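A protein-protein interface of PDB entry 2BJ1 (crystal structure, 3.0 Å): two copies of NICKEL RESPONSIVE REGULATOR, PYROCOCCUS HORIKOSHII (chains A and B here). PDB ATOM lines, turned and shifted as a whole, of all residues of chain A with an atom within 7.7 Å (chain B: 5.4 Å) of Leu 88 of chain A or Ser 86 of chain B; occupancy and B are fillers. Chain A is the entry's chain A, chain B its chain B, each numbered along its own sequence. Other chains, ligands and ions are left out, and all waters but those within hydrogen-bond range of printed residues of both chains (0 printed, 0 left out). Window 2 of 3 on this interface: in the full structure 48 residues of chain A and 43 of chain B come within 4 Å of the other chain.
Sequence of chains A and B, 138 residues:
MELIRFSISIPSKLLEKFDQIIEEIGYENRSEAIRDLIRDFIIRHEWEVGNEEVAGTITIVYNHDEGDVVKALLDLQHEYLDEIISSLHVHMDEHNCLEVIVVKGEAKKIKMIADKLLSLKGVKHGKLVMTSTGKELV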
ATOM      1  N   ILE A  58     -25.837  -7.589 -20.103  1.00  0.00           N
ATOM      2  CA  ILE A  58     -25.383  -7.753 -21.480  1.00  0.00           C
ATOM      3  C   ILE A  58     -23.905  -8.159 -21.378  1.00  0.00           C
ATOM      4  O   ILE A  58     -23.042  -7.310 -21.191  1.00  0.00           O
ATOM      5  CB  ILE A  58     -25.424  -6.436 -22.279  1.00  0.00           C
ATOM      6  CG1 ILE A  58     -26.851  -5.918 -22.415  1.00  0.00           C
ATOM      7  CG2 ILE A  58     -24.824  -6.656 -23.663  1.00  0.00           C
ATOM      8  CD1 ILE A  58     -26.948  -4.618 -23.250  1.00  0.00           C
ATOM      9  N   ILE A  60     -20.325  -9.350 -22.832  1.00  0.00           N
ATOM     10  CA  ILE A  60     -19.584  -9.302 -24.092  1.00  0.00           C
ATOM     11  C   ILE A  60     -18.105  -9.597 -23.887  1.00  0.00           C
ATOM     12  O   ILE A  60     -17.618  -9.623 -22.756  1.00  0.00           O
ATOM     13  CB  ILE A  60     -19.732  -7.946 -24.800  1.00  0.00           C
ATOM     14  CG1 ILE A  60     -18.940  -6.865 -24.071  1.00  0.00           C
ATOM     15  CG2 ILE A  60     -21.190  -7.583 -24.873  1.00  0.00           C
ATOM     16  CD1 ILE A  60     -18.944  -5.512 -24.772  1.00  0.00           C
ATOM     17  N   TYR A  62     -14.113  -8.806 -25.795  1.00  0.00           N
ATOM     18  CA  TYR A  62     -13.390  -8.095 -26.832  1.00  0.00           C
ATOM     19  C   TYR A  62     -11.876  -8.060 -26.676  1.00  0.00           C
ATOM     20  O   TYR A  62     -11.305  -8.704 -25.803  1.00  0.00           O
ATOM     21  CB  TYR A  62     -13.940  -6.667 -26.969  1.00  0.00           C
ATOM     22  CG  TYR A  62     -13.971  -5.829 -25.701  1.00  0.00           C
ATOM     23  CD1 TYR A  62     -12.799  -5.333 -25.128  1.00  0.00           C
ATOM     24  CD2 TYR A  62     -15.185  -5.482 -25.102  1.00  0.00           C
ATOM     25  CE1 TYR A  62     -12.833  -4.505 -23.994  1.00  0.00           C
ATOM     26  CE2 TYR A  62     -15.232  -4.660 -23.969  1.00  0.00           C
ATOM     27  CZ  TYR A  62     -14.053  -4.173 -23.423  1.00  0.00           C
ATOM     28  OH  TYR A  62     -14.099  -3.346 -22.320  1.00  0.00           O
ATOM     29  N   SER A  86     -24.382   0.072 -14.493  1.00  0.00           N
ATOM     30  CA  SER A  86     -22.971  -0.138 -14.180  1.00  0.00           C
ATOM     31  C   SER A  86     -22.457  -1.244 -15.065  1.00  0.00           C
ATOM     32  O   SER A  86     -23.204  -1.772 -15.877  1.00  0.00           O
ATOM     33  CB  SER A  86     -22.813  -0.578 -12.739  1.00  0.00           C
ATOM     34  OG  SER A  86     -23.420   0.357 -11.883  1.00  0.00           O
ATOM     35  N   SER A  87     -21.194  -1.613 -14.904  1.00  0.00           N
ATOM     36  CA  SER A  87     -20.649  -2.686 -15.715  1.00  0.00           C
ATOM     37  C   SER A  87     -19.348  -3.215 -15.169  1.00  0.00           C
ATOM     38  O   SER A  87     -18.397  -2.479 -15.011  1.00  0.00           O
ATOM     39  CB  SER A  87     -20.427  -2.217 -17.143  1.00  0.00           C
ATOM     40  OG  SER A  87     -19.241  -1.462 -17.230  1.00  0.00           O
ATOM     41  N   LEU A  88     -19.318  -4.510 -14.898  1.00  0.00           N
ATOM     42  CA  LEU A  88     -18.133  -5.165 -14.374  1.00  0.00           C
ATOM     43  C   LEU A  88     -17.233  -5.531 -15.544  1.00  0.00           C
ATOM     44  O   LEU A  88     -17.714  -5.873 -16.607  1.00  0.00           O
ATOM     45  CB  LEU A  88     -18.536  -6.418 -13.596  1.00  0.00           C
ATOM     46  CG  LEU A  88     -17.447  -7.049 -12.734  1.00  0.00           C
ATOM     47  CD1 LEU A  88     -16.700  -5.976 -11.954  1.00  0.00           C
ATOM     48  CD2 LEU A  88     -18.072  -8.042 -11.797  1.00  0.00           C
ATOM     49  N   HIS A  89     -15.925  -5.462 -15.343  1.00  0.00           N
ATOM     50  CA  HIS A  89     -14.976  -5.762 -16.403  1.00  0.00           C
ATOM     51  C   HIS A  89     -13.773  -6.531 -15.900  1.00  0.00           C
ATOM     52  O   HIS A  89     -12.955  -6.020 -15.155  1.00  0.00           O
ATOM     53  CB  HIS A  89     -14.543  -4.445 -17.071  1.00  0.00           C
ATOM     54  CG  HIS A  89     -13.362  -4.560 -17.992  1.00  0.00           C
ATOM     55  ND1 HIS A  89     -13.063  -3.588 -18.927  1.00  0.00           N
ATOM     56  CD2 HIS A  89     -12.364  -5.474 -18.073  1.00  0.00           C
ATOM     57  CE1 HIS A  89     -11.933  -3.896 -19.538  1.00  0.00           C
ATOM     58  NE2 HIS A  89     -11.487  -5.036 -19.038  1.00  0.00           N
ATOM     59  N   VAL A  90     -13.670  -7.773 -16.331  1.00  0.00           N
ATOM     60  CA  VAL A  90     -12.551  -8.617 -15.963  1.00  0.00           C
ATOM     61  C   VAL A  90     -11.557  -8.653 -17.130  1.00  0.00           C
ATOM     62  O   VAL A  90     -11.956  -8.649 -18.289  1.00  0.00           O
ATOM     63  CB  VAL A  90     -13.019 -10.064 -15.657  1.00  0.00           C
ATOM     64  CG1 VAL A  90     -11.816 -10.988 -15.507  1.00  0.00           C
ATOM     65  CG2 VAL A  90     -13.872 -10.080 -14.390  1.00  0.00           C
ATOM     66  N   LEU A  98     -13.527  -9.140 -20.739  1.00  0.00           N
ATOM     67  CA  LEU A  98     -14.830  -9.704 -20.423  1.00  0.00           C
ATOM     68  C   LEU A  98     -15.553  -8.557 -19.704  1.00  0.00           C
ATOM     69  O   LEU A  98     -15.055  -8.037 -18.716  1.00  0.00           O
ATOM     70  CB  LEU A  98     -14.684 -10.898 -19.479  1.00  0.00           C
ATOM     71  CG  LEU A  98     -15.858 -11.881 -19.484  1.00  0.00           C
ATOM     72  CD1 LEU A  98     -15.772 -12.778 -18.262  1.00  0.00           C
ATOM     73  CD2 LEU A  98     -17.173 -11.124 -19.491  1.00  0.00           C
ATOM     74  N   GLU A  99     -16.711  -8.147 -20.195  1.00  0.00           N
ATOM     75  CA  GLU A  99     -17.413  -7.048 -19.554  1.00  0.00           C
ATOM     76  C   GLU A  99     -18.925  -7.253 -19.486  1.00  0.00           C
ATOM     77  O   GLU A  99     -19.586  -7.337 -20.513  1.00  0.00           O
ATOM     78  CB  GLU A  99     -17.093  -5.740 -20.292  1.00  0.00           C
ATOM     79  CG  GLU A  99     -17.737  -4.498 -19.695  1.00  0.00           C
ATOM     80  CD  GLU A  99     -17.241  -3.196 -20.316  1.00  0.00           C
ATOM     81  OE1 GLU A  99     -16.029  -2.900 -20.211  1.00  0.00           O
ATOM     82  OE2 GLU A  99     -18.069  -2.463 -20.903  1.00  0.00           O
ATOM     83  N   VAL A 100     -19.462  -7.340 -18.269  1.00  0.00           N
ATOM     84  CA  VAL A 100     -20.899  -7.511 -18.052  1.00  0.00           C
ATOM     85  C   VAL A 100     -21.538  -6.141 -17.855  1.00  0.00           C
ATOM     86  O   VAL A 100     -21.224  -5.461 -16.886  1.00  0.00           O
ATOM     87  CB  VAL A 100     -21.192  -8.298 -16.769  1.00  0.00           C
ATOM     88  CG1 VAL A 100     -22.662  -8.660 -16.721  1.00  0.00           C
ATOM     89  CG2 VAL A 100     -20.335  -9.523 -16.698  1.00  0.00           C
ATOM     90  N   ILE A 101     -22.436  -5.735 -18.747  1.00  0.00           N
ATOM     91  CA  ILE A 101     -23.089  -4.433 -18.605  1.00  0.00           C
ATOM     92  C   ILE A 101     -24.512  -4.596 -18.069  1.00  0.00           C
ATOM     93  O   ILE A 101     -25.336  -5.256 -18.699  1.00  0.00           O
ATOM     94  CB  ILE A 101     -23.167  -3.707 -19.950  1.00  0.00           C
ATOM     95  CG1 ILE A 101     -21.787  -3.673 -20.594  1.00  0.00           C
ATOM     96  CG2 ILE A 101     -23.706  -2.300 -19.759  1.00  0.00           C
ATOM     97  CD1 ILE A 101     -21.796  -3.038 -21.933  1.00  0.00           C
ATOM     98  N   VAL A 102     -24.796  -4.001 -16.907  1.00  0.00           N
ATOM     99  CA  VAL A 102     -26.129  -4.085 -16.295  1.00  0.00           C
ATOM    100  C   VAL A 102     -27.013  -2.940 -16.770  1.00  0.00           C
ATOM    101  O   VAL A 102     -26.610  -1.775 -16.738  1.00  0.00           O
ATOM    102  CB  VAL A 102     -26.071  -4.028 -14.767  1.00  0.00           C
ATOM    103  CG1 VAL A 102     -27.452  -4.267 -14.207  1.00  0.00           C
ATOM    104  CG2 VAL A 102     -25.101  -5.065 -14.241  1.00  0.00           C
ATOM    105  N   ILE B  84     -14.694 -18.251  -8.032  1.00  0.00           N
ATOM    106  CA  ILE B  84     -15.424 -16.993  -8.040  1.00  0.00           C
ATOM    107  C   ILE B  84     -14.484 -15.793  -7.877  1.00  0.00           C
ATOM    108  O   ILE B  84     -13.838 -15.613  -6.839  1.00  0.00           O
ATOM    109  CB  ILE B  84     -16.503 -16.972  -6.948  1.00  0.00           C
ATOM    110  CG1 ILE B  84     -17.635 -17.918  -7.340  1.00  0.00           C
ATOM    111  CG2 ILE B  84     -17.042 -15.582  -6.783  1.00  0.00           C
ATOM    112  CD1 ILE B  84     -18.794 -17.945  -6.371  1.00  0.00           C
ATOM    113  N   ILE B  85     -14.424 -14.990  -8.934  1.00  0.00           N
ATOM    114  CA  ILE B  85     -13.604 -13.789  -9.020  1.00  0.00           C
ATOM    115  C   ILE B  85     -14.166 -12.651  -8.179  1.00  0.00           C
ATOM    116  O   ILE B  85     -13.612 -12.306  -7.137  1.00  0.00           O
ATOM    117  CB  ILE B  85     -13.528 -13.362 -10.468  1.00  0.00           C
ATOM    118  CG1 ILE B  85     -12.738 -14.414 -11.239  1.00  0.00           C
ATOM    119  CG2 ILE B  85     -12.913 -12.002 -10.587  1.00  0.00           C
ATOM    120  CD1 ILE B  85     -13.052 -14.463 -12.701  1.00  0.00           C
ATOM    121  N   SER B  86     -15.257 -12.057  -8.647  1.00  0.00           N
ATOM    122  CA  SER B  86     -15.914 -10.982  -7.914  1.00  0.00           C
ATOM    123  C   SER B  86     -17.397 -10.986  -8.273  1.00  0.00           C
ATOM    124  O   SER B  86     -17.821 -11.757  -9.128  1.00  0.00           O
ATOM    125  CB  SER B  86     -15.268  -9.636  -8.238  1.00  0.00           C
ATOM    126  OG  SER B  86     -15.214  -9.417  -9.629  1.00  0.00           O
ATOM    127  N   SER B  87     -18.189 -10.138  -7.632  1.00  0.00           N
ATOM    128  CA  SER B  87     -19.616 -10.130  -7.907  1.00  0.00           C
ATOM    129  C   SER B  87     -20.276  -8.755  -7.879  1.00  0.00           C
ATOM    130  O   SER B  87     -20.138  -8.011  -6.915  1.00  0.00           O
ATOM    131  CB  SER B  87     -20.316 -11.054  -6.911  1.00  0.00           C
ATOM    132  OG  SER B  87     -21.542 -10.493  -6.461  1.00  0.00           O
ATOM    133  N   LEU B  88     -21.006  -8.428  -8.941  1.00  0.00           N
ATOM    134  CA  LEU B  88     -21.694  -7.150  -9.028  1.00  0.00           C
ATOM    135  C   LEU B  88     -23.139  -7.349  -8.609  1.00  0.00           C
ATOM    136  O   LEU B  88     -23.793  -8.276  -9.068  1.00  0.00           O
ATOM    137  CB  LEU B  88     -21.633  -6.610 -10.449  1.00  0.00           C
ATOM    138  CG  LEU B  88     -22.412  -5.313 -10.644  1.00  0.00           C
ATOM    139  CD1 LEU B  88     -22.030  -4.327  -9.550  1.00  0.00           C
ATOM    140  CD2 LEU B  88     -22.127  -4.727 -12.012  1.00  0.00           C
ATOM    141  N   VAL B 100     -24.759 -10.201 -10.788  1.00  0.00           N
ATOM    142  CA  VAL B 100     -24.007 -10.967 -11.770  1.00  0.00           C
ATOM    143  C   VAL B 100     -22.664 -11.392 -11.154  1.00  0.00           C
ATOM    144  O   VAL B 100     -21.812 -10.567 -10.835  1.00  0.00           O
ATOM    145  CB  VAL B 100     -23.820 -10.161 -13.088  1.00  0.00           C
ATOM    146  CG1 VAL B 100     -23.681  -8.685 -12.795  1.00  0.00           C
ATOM    147  CG2 VAL B 100     -22.613 -10.675 -13.846  1.00  0.00           C
ATOM    148  N   ILE B 101     -22.511 -12.699 -10.969  1.00  0.00           N
ATOM    149  CA  ILE B 101     -21.318 -13.296 -10.372  1.00  0.00           C
ATOM    150  C   ILE B 101     -20.296 -13.772 -11.401  1.00  0.00           C
ATOM    151  O   ILE B 101     -20.579 -14.700 -12.143  1.00  0.00           O
ATOM    152  CB  ILE B 101     -21.710 -14.510  -9.552  1.00  0.00           C
ATOM    153  CG1 ILE B 101     -22.909 -14.160  -8.678  1.00  0.00           C
ATOM    154  CG2 ILE B 101     -20.542 -14.967  -8.719  1.00  0.00           C
ATOM    155  CD1 ILE B 101     -23.477 -15.344  -7.927  1.00  0.00           C
ATOM    156  N   VAL B 102     -19.111 -13.166 -11.438  1.00  0.00           N
ATOM    157  CA  VAL B 102     -18.080 -13.584 -12.394  1.00  0.00           C
ATOM    158  C   VAL B 102     -17.286 -14.796 -11.911  1.00  0.00           C
ATOM    159  O   VAL B 102     -16.773 -14.815 -10.799  1.00  0.00           O
ATOM    160  CB  VAL B 102     -17.083 -12.461 -12.690  1.00  0.00           C
ATOM    161  CG1 VAL B 102     -15.947 -13.005 -13.542  1.00  0.00           C
ATOM    162  CG2 VAL B 102     -17.791 -11.316 -13.412  1.00  0.00           C
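The backbone carbonyl oxygen (O) of Ser 86 of chain A lies within hydrogen-bond range of the backbone NH (N) of Val 102 of chain A (2.9 Å). The backbone NH (N) of Ile 85 of chain B lies within hydrogen-bond range of the backbone carbonyl oxygen (O) of Val 102 of chain B (3.0 Å). N of Val 100 of chain B sits at hydrogen-bond distance from O of Leu 88 of chain B, at 2.8 Å. The backbone NH (N) of Val 102 of chain B is in hydrogen-bond range of the backbone carbonyl oxygen (O) of Ser 86 of chain B (3.0 Å). N of Val 90 of chain A lies within hydrogen-bond range of O of Leu 98 of chain A, 2.8 Å away. The backbone carbonyl oxygen (O) of Leu 88 of chain A is in hydrogen-bond range of the backbone NH (N) of Val 100 of chain A, 2.8 Å away.
Leu 88 of chain A touches Ser 86 of chain B (CD2 to OG, 3.8 Å). CD2 of Leu 88 of chain A touches CG2 of Val 102 of chain B (3.7 Å). CG2 of Val 90 of chain A touches CG1 of Val 102 of chain B (3.7 Å). CG1 of Val 100 of chain A touches CG2 of Val 100 of chain B (3.5 Å). Val 102 of chain A touches Leu 88 of chain B (CG2 to CD2, 3.7 Å).
Leu 88 of chain A touches just these residues of chain B: Ser 86 and Val 102. Leu 98 of chain A touches none of the printed residues of chain B. Of the printed residues of chain B, Val 100 of chain A touches Val 100 (3.5 Å). Printed residues of chain B within 4 Å of Val 102 of chain A: Leu 88 (3.7 Å). Of chain A, only Leu 88 (3.8 Å) comes within 4 Å of Ser 86 of chain B. Printed residues of chain A within 4 Å of Leu 88 of chain B: Val 102. Of the printed residues of chain A, Val 100 of chain B touches Val 100 (3.5 Å). Ile 101 of chain B touches none of the printed residues of chain A. Printed residues of chain A within 4 Å of Val 102 of chain B: Leu 88 (3.7 Å) and Val 90 (3.7 Å). The nearest residue of chain B that does not touch Leu 88 of chain A is Leu 88 of chain B (4.03 Å). The nearest printed residue of chain B that does not touch Val 90 of chain A is Ile 85 of chain B (4.4 Å).
Printed residues of chain A that touch a printed residue of chain B: Leu 88, Val 90, Val 100 and Val 102. Hydrophobic or aromatic side chains of chain A within 4 Å of the printed part of chain B: Leu 88, Val 90, Val 100 and Val 102. Of the 8 printed residues of chain B, 4 touch a printed residue of chain A. Hydrophobic or aromatic side chains of chain B that line the printed part of chain A: Leu 88, Val 100 and Val 102. Among the printed residues, no Asp or Glu carboxylate lies within 4 Å of a Lys or Arg side-chain nitrogen of the other chain.
Leu 88 of chain A touches Ser 86 of chain B, but with the chains exchanged Ser 86 of chain A does not touch Leu 88 of chain B (4.3 Å). Leu 88 of chain A touches Val 102 of chain B, and with the chains exchanged Val 102 of chain A touches Leu 88 of chain B. Val 100 of chain A touches its own counterpart, Val 100 of chain B. Positions printed for both chains: 86, 87, 88, 100, 101 and 102.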
